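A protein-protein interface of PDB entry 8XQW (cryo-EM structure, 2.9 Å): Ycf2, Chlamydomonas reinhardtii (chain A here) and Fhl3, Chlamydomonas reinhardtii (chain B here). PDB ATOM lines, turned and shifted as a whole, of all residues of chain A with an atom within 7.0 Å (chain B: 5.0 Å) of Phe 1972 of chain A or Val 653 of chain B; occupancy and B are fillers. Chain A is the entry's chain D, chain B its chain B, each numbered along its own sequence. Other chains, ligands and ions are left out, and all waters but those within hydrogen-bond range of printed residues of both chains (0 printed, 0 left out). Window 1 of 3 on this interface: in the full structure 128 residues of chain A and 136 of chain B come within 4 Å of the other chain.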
ATOM      1  N   THR A1954       1.237 -10.700  15.014  1.00  0.00           N
ATOM      2  CA  THR A1954       1.326 -12.091  15.436  1.00  0.00           C
ATOM      3  C   THR A1954       2.740 -12.378  15.910  1.00  0.00           C
ATOM      4  O   THR A1954       3.707 -12.108  15.199  1.00  0.00           O
ATOM      5  CB  THR A1954       0.946 -13.041  14.312  1.00  0.00           C
ATOM      6  OG1 THR A1954      -0.268 -12.587  13.705  1.00  0.00           O
ATOM      7  CG2 THR A1954       0.723 -14.421  14.859  1.00  0.00           C
ATOM      8  N   TYR A1955       2.855 -12.930  17.112  1.00  0.00           N
ATOM      9  CA  TYR A1955       4.117 -12.945  17.828  1.00  0.00           C
ATOM     10  C   TYR A1955       4.300 -14.292  18.505  1.00  0.00           C
ATOM     11  O   TYR A1955       3.331 -15.000  18.770  1.00  0.00           O
ATOM     12  CB  TYR A1955       4.145 -11.825  18.861  1.00  0.00           C
ATOM     13  CG  TYR A1955       5.510 -11.360  19.250  1.00  0.00           C
ATOM     14  CD1 TYR A1955       6.316 -10.695  18.349  1.00  0.00           C
ATOM     15  CD2 TYR A1955       5.989 -11.561  20.528  1.00  0.00           C
ATOM     16  CE1 TYR A1955       7.569 -10.263  18.705  1.00  0.00           C
ATOM     17  CE2 TYR A1955       7.240 -11.129  20.895  1.00  0.00           C
ATOM     18  CZ  TYR A1955       8.026 -10.483  19.980  1.00  0.00           C
ATOM     19  OH  TYR A1955       9.275 -10.048  20.343  1.00  0.00           O
ATOM     20  N   GLN A1956       5.549 -14.643  18.780  1.00  0.00           N
ATOM     21  CA  GLN A1956       5.883 -15.854  19.524  1.00  0.00           C
ATOM     22  C   GLN A1956       6.531 -15.417  20.826  1.00  0.00           C
ATOM     23  O   GLN A1956       7.643 -14.879  20.818  1.00  0.00           O
ATOM     24  CB  GLN A1956       6.799 -16.761  18.711  1.00  0.00           C
ATOM     25  CG  GLN A1956       6.190 -17.186  17.387  1.00  0.00           C
ATOM     26  CD  GLN A1956       6.311 -18.672  17.139  1.00  0.00           C
ATOM     27  OE1 GLN A1956       5.317 -19.355  16.901  1.00  0.00           O
ATOM     28  NE2 GLN A1956       7.534 -19.184  17.191  1.00  0.00           N
ATOM     29  N   SER A1957       5.846 -15.656  21.942  1.00  0.00           N
ATOM     30  CA  SER A1957       6.064 -14.857  23.139  1.00  0.00           C
ATOM     31  C   SER A1957       6.543 -15.683  24.324  1.00  0.00           C
ATOM     32  O   SER A1957       6.078 -16.801  24.555  1.00  0.00           O
ATOM     33  CB  SER A1957       4.783 -14.112  23.526  1.00  0.00           C
ATOM     34  OG  SER A1957       5.072 -12.846  24.098  1.00  0.00           O
ATOM     35  N   LEU A1971       4.107 -19.786  20.175  1.00  0.00           N
ATOM     36  CA  LEU A1971       2.752 -20.089  20.604  1.00  0.00           C
ATOM     37  C   LEU A1971       1.748 -19.233  19.847  1.00  0.00           C
ATOM     38  O   LEU A1971       0.553 -19.493  19.890  1.00  0.00           O
ATOM     39  CB  LEU A1971       2.613 -19.884  22.109  1.00  0.00           C
ATOM     40  CG  LEU A1971       1.408 -20.536  22.780  1.00  0.00           C
ATOM     41  CD1 LEU A1971       1.120 -21.881  22.155  1.00  0.00           C
ATOM     42  CD2 LEU A1971       1.640 -20.680  24.266  1.00  0.00           C
ATOM     43  N   PHE A1972       2.244 -18.217  19.144  1.00  0.00           N
ATOM     44  CA  PHE A1972       1.443 -17.418  18.219  1.00  0.00           C
ATOM     45  C   PHE A1972       0.308 -16.685  18.936  1.00  0.00           C
ATOM     46  O   PHE A1972      -0.873 -16.978  18.764  1.00  0.00           O
ATOM     47  CB  PHE A1972       0.882 -18.288  17.095  1.00  0.00           C
ATOM     48  CG  PHE A1972       1.902 -18.707  16.101  1.00  0.00           C
ATOM     49  CD1 PHE A1972       2.721 -17.770  15.503  1.00  0.00           C
ATOM     50  CD2 PHE A1972       2.046 -20.036  15.761  1.00  0.00           C
ATOM     51  CE1 PHE A1972       3.659 -18.151  14.584  1.00  0.00           C
ATOM     52  CE2 PHE A1972       2.984 -20.424  14.843  1.00  0.00           C
ATOM     53  CZ  PHE A1972       3.791 -19.483  14.252  1.00  0.00           C
ATOM     54  N   ILE A1973       0.712 -15.723  19.759  1.00  0.00           N
ATOM     55  CA  ILE A1973      -0.226 -14.749  20.290  1.00  0.00           C
ATOM     56  C   ILE A1973      -0.577 -13.740  19.207  1.00  0.00           C
ATOM     57  O   ILE A1973       0.280 -13.343  18.411  1.00  0.00           O
ATOM     58  CB  ILE A1973       0.394 -14.059  21.510  1.00  0.00           C
ATOM     59  CG1 ILE A1973       1.038 -15.101  22.408  1.00  0.00           C
ATOM     60  CG2 ILE A1973      -0.640 -13.296  22.264  1.00  0.00           C
ATOM     61  CD1 ILE A1973       1.245 -14.636  23.803  1.00  0.00           C
ATOM     62  N   ASP A1974      -1.839 -13.322  19.157  1.00  0.00           N
ATOM     63  CA  ASP A1974      -2.252 -12.220  18.297  1.00  0.00           C
ATOM     64  C   ASP A1974      -2.543 -10.998  19.144  1.00  0.00           C
ATOM     65  O   ASP A1974      -3.357 -11.058  20.066  1.00  0.00           O
ATOM     66  CB  ASP A1974      -3.489 -12.564  17.480  1.00  0.00           C
ATOM     67  CG  ASP A1974      -3.343 -13.846  16.728  1.00  0.00           C
ATOM     68  OD1 ASP A1974      -2.217 -14.377  16.692  1.00  0.00           O
ATOM     69  OD2 ASP A1974      -4.353 -14.328  16.175  1.00  0.00           O
ATOM     70  N   ILE A2048      -4.958 -12.519  22.043  1.00  0.00           N
ATOM     71  CA  ILE A2048      -5.738 -13.741  21.971  1.00  0.00           C
ATOM     72  C   ILE A2048      -4.858 -14.876  21.474  1.00  0.00           C
ATOM     73  O   ILE A2048      -3.965 -14.682  20.644  1.00  0.00           O
ATOM     74  CB  ILE A2048      -6.976 -13.547  21.075  1.00  0.00           C
ATOM     75  CG1 ILE A2048      -7.830 -14.804  21.047  1.00  0.00           C
ATOM     76  CG2 ILE A2048      -6.570 -13.156  19.690  1.00  0.00           C
ATOM     77  CD1 ILE A2048      -9.036 -14.668  20.201  1.00  0.00           C
ATOM     78  N   ILE A2049      -5.090 -16.066  22.012  1.00  0.00           N
ATOM     79  CA  ILE A2049      -4.356 -17.263  21.635  1.00  0.00           C
ATOM     80  C   ILE A2049      -5.356 -18.303  21.166  1.00  0.00           C
ATOM     81  O   ILE A2049      -6.362 -18.548  21.837  1.00  0.00           O
ATOM     82  CB  ILE A2049      -3.521 -17.804  22.802  1.00  0.00           C
ATOM     83  CG1 ILE A2049      -2.825 -16.649  23.503  1.00  0.00           C
ATOM     84  CG2 ILE A2049      -2.527 -18.804  22.305  1.00  0.00           C
ATOM     85  CD1 ILE A2049      -1.884 -17.069  24.570  1.00  0.00           C
ATOM     86  N   THR A2050      -5.080 -18.913  20.024  1.00  0.00           N
ATOM     87  CA  THR A2050      -5.998 -19.853  19.408  1.00  0.00           C
ATOM     88  C   THR A2050      -5.284 -21.165  19.142  1.00  0.00           C
ATOM     89  O   THR A2050      -4.111 -21.185  18.769  1.00  0.00           O
ATOM     90  CB  THR A2050      -6.561 -19.304  18.099  1.00  0.00           C
ATOM     91  OG1 THR A2050      -6.968 -17.945  18.285  1.00  0.00           O
ATOM     92  CG2 THR A2050      -7.753 -20.119  17.656  1.00  0.00           C
ATOM     93  N   ASN B 649       5.737 -25.169  11.188  1.00  0.00           N
ATOM     94  CA  ASN B 649       5.769 -23.939  11.971  1.00  0.00           C
ATOM     95  C   ASN B 649       6.582 -22.868  11.264  1.00  0.00           C
ATOM     96  O   ASN B 649       6.271 -21.677  11.355  1.00  0.00           O
ATOM     97  CB  ASN B 649       6.329 -24.198  13.366  1.00  0.00           C
ATOM     98  CG  ASN B 649       5.544 -25.240  14.122  1.00  0.00           C
ATOM     99  OD1 ASN B 649       6.115 -26.160  14.706  1.00  0.00           O
ATOM    100  ND2 ASN B 649       4.224 -25.115  14.104  1.00  0.00           N
ATOM    101  N   GLU B 650       7.624 -23.274  10.541  1.00  0.00           N
ATOM    102  CA  GLU B 650       8.417 -22.294   9.812  1.00  0.00           C
ATOM    103  C   GLU B 650       7.646 -21.731   8.631  1.00  0.00           C
ATOM    104  O   GLU B 650       7.706 -20.527   8.360  1.00  0.00           O
ATOM    105  CB  GLU B 650       9.727 -22.914   9.348  1.00  0.00           C
ATOM    106  CG  GLU B 650      10.810 -21.893   9.149  1.00  0.00           C
ATOM    107  CD  GLU B 650      11.009 -21.035  10.373  1.00  0.00           C
ATOM    108  OE1 GLU B 650      11.062 -21.596  11.490  1.00  0.00           O
ATOM    109  OE2 GLU B 650      11.104 -19.798  10.223  1.00  0.00           O
ATOM    110  N   LEU B 651       6.917 -22.585   7.915  1.00  0.00           N
ATOM    111  CA  LEU B 651       6.059 -22.092   6.846  1.00  0.00           C
ATOM    112  C   LEU B 651       5.058 -21.079   7.384  1.00  0.00           C
ATOM    113  O   LEU B 651       4.826 -20.029   6.774  1.00  0.00           O
ATOM    114  CB  LEU B 651       5.349 -23.262   6.175  1.00  0.00           C
ATOM    115  CG  LEU B 651       5.083 -23.100   4.682  1.00  0.00           C
ATOM    116  CD1 LEU B 651       6.303 -22.547   3.998  1.00  0.00           C
ATOM    117  CD2 LEU B 651       4.703 -24.428   4.083  1.00  0.00           C
ATOM    118  N   LEU B 652       4.465 -21.373   8.541  1.00  0.00           N
ATOM    119  CA  LEU B 652       3.548 -20.423   9.163  1.00  0.00           C
ATOM    120  C   LEU B 652       4.245 -19.106   9.465  1.00  0.00           C
ATOM    121  O   LEU B 652       3.811 -18.044   9.009  1.00  0.00           O
ATOM    122  CB  LEU B 652       2.967 -21.015  10.440  1.00  0.00           C
ATOM    123  CG  LEU B 652       2.147 -22.279  10.238  1.00  0.00           C
ATOM    124  CD1 LEU B 652       1.698 -22.820  11.576  1.00  0.00           C
ATOM    125  CD2 LEU B 652       0.968 -21.991   9.344  1.00  0.00           C
ATOM    126  N   VAL B 653       5.332 -19.157  10.238  1.00  0.00           N
ATOM    127  CA  VAL B 653       6.042 -17.944  10.630  1.00  0.00           C
ATOM    128  C   VAL B 653       6.422 -17.110   9.417  1.00  0.00           C
ATOM    129  O   VAL B 653       6.394 -15.876   9.470  1.00  0.00           O
ATOM    130  CB  VAL B 653       7.283 -18.294  11.470  1.00  0.00           C
ATOM    131  CG1 VAL B 653       8.102 -17.054  11.739  1.00  0.00           C
ATOM    132  CG2 VAL B 653       6.876 -18.932  12.769  1.00  0.00           C
ATOM    133  N   GLN B 654       6.779 -17.752   8.310  1.00  0.00           N
ATOM    134  CA  GLN B 654       7.129 -16.995   7.119  1.00  0.00           C
ATOM    135  C   GLN B 654       5.917 -16.440   6.394  1.00  0.00           C
ATOM    136  O   GLN B 654       6.022 -15.388   5.760  1.00  0.00           O
ATOM    137  CB  GLN B 654       7.941 -17.860   6.157  1.00  0.00           C
ATOM    138  CG  GLN B 654       9.268 -18.293   6.720  1.00  0.00           C
ATOM    139  CD  GLN B 654      10.027 -17.150   7.344  1.00  0.00           C
ATOM    140  OE1 GLN B 654      10.119 -16.063   6.777  1.00  0.00           O
ATOM    141  NE2 GLN B 654      10.580 -17.389   8.524  1.00  0.00           N
ATOM    142  N   MET B 655       4.773 -17.109   6.481  1.00  0.00           N
ATOM    143  CA  MET B 655       3.581 -16.591   5.825  1.00  0.00           C
ATOM    144  C   MET B 655       2.830 -15.592   6.700  1.00  0.00           C
ATOM    145  O   MET B 655       2.117 -14.729   6.183  1.00  0.00           O
ATOM    146  CB  MET B 655       2.659 -17.746   5.432  1.00  0.00           C
ATOM    147  CG  MET B 655       3.239 -18.656   4.382  1.00  0.00           C
ATOM    148  SD  MET B 655       3.047 -17.987   2.730  1.00  0.00           S
ATOM    149  CE  MET B 655       1.322 -18.334   2.448  1.00  0.00           C
ATOM    150  N   ASP B 656       2.962 -15.700   8.025  1.00  0.00           N
ATOM    151  CA  ASP B 656       2.154 -14.894   8.927  1.00  0.00           C
ATOM    152  C   ASP B 656       2.921 -13.934   9.820  1.00  0.00           C
ATOM    153  O   ASP B 656       2.673 -12.728   9.738  1.00  0.00           O
ATOM    154  CB  ASP B 656       1.311 -15.794   9.842  1.00  0.00           C
ATOM    155  CG  ASP B 656       0.657 -16.936   9.100  1.00  0.00           C
ATOM    156  OD1 ASP B 656       0.518 -16.843   7.864  1.00  0.00           O
ATOM    157  OD2 ASP B 656       0.270 -17.923   9.757  1.00  0.00           O
ATOM    158  N   GLY B 657       3.853 -14.415  10.638  1.00  0.00           N
ATOM    159  CA  GLY B 657       4.313 -13.695  11.812  1.00  0.00           C
ATOM    160  C   GLY B 657       4.728 -12.252  11.624  1.00  0.00           C
ATOM    161  O   GLY B 657       4.025 -11.338  12.061  1.00  0.00           O
ATOM    162  N   PHE B 658       5.853 -12.027  10.959  1.00  0.00           N
ATOM    163  CA  PHE B 658       6.356 -10.684  10.697  1.00  0.00           C
ATOM    164  C   PHE B 658       6.550 -10.502   9.210  1.00  0.00           C
ATOM    165  O   PHE B 658       7.604 -10.076   8.734  1.00  0.00           O
ATOM    166  CB  PHE B 658       7.652 -10.416  11.445  1.00  0.00           C
ATOM    167  CG  PHE B 658       7.451  -9.812  12.793  1.00  0.00           C
ATOM    168  CD1 PHE B 658       6.829 -10.527  13.793  1.00  0.00           C
ATOM    169  CD2 PHE B 658       7.883  -8.528  13.061  1.00  0.00           C
ATOM    170  CE1 PHE B 658       6.643  -9.974  15.038  1.00  0.00           C
ATOM    171  CE2 PHE B 658       7.700  -7.968  14.308  1.00  0.00           C
ATOM    172  CZ  PHE B 658       7.080  -8.692  15.298  1.00  0.00           C
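The backbone carbonyl oxygen of Thr 1954 of chain A sits close to the backbone carbonyl oxygen of Gly 657 of chain B.
N of Ile 1973 of chain A is in hydrogen-bond range of O of Tyr 1955 of chain A, 2.9 Å away.
The backbone carbonyl oxygen of Tyr 1955 of chain A lies close to the backbone NH of Phe 1972 of chain A (3.4 Å).
O of Thr 1954 of chain A touches CE1 of Phe 658 of chain B (3.6 Å).
Phe 658 of chain B touches Tyr 1955 of chain A (CE1 to CD1, 3.4 Å).
CZ of Phe 1972 of chain A touches CG2 of Val 653 of chain B, at 3.5 Å.
Val 653 of chain B touches just one residue of chain A: Phe 1972 (3.5 Å).
Of the printed residues of chain B, Thr 1954 of chain A touches Gly 657 (3.2 Å) and Phe 658 (3.6 Å).
Of the printed residues of chain B, Tyr 1955 of chain A touches Phe 658 (3.4 Å).
Printed residues of chain A within 4 Å of Phe 658 of chain B: Thr 1954 (3.6 Å) and Tyr 1955 (3.4 Å).
Of the printed residues of chain A, Gly 657 of chain B touches Thr 1954.
The nearest residue of chain B that does not touch Phe 1972 of chain A is Leu 652 of chain B (4.2 Å).
The nearest residue of chain A that does not touch Val 653 of chain B is Gln 1956 of chain A (4.4 Å).
Printed residues of chain A that touch a printed residue of chain B: Thr 1954, Tyr 1955 and Phe 1972.
Of the 10 printed residues of chain B, 3 touch a printed residue of chain A.
Hydrophobic or aromatic side chains of chain B that line the printed part of chain A: Val 653 and Phe 658.
Among the printed residues, 4 pairs touch across the chains.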
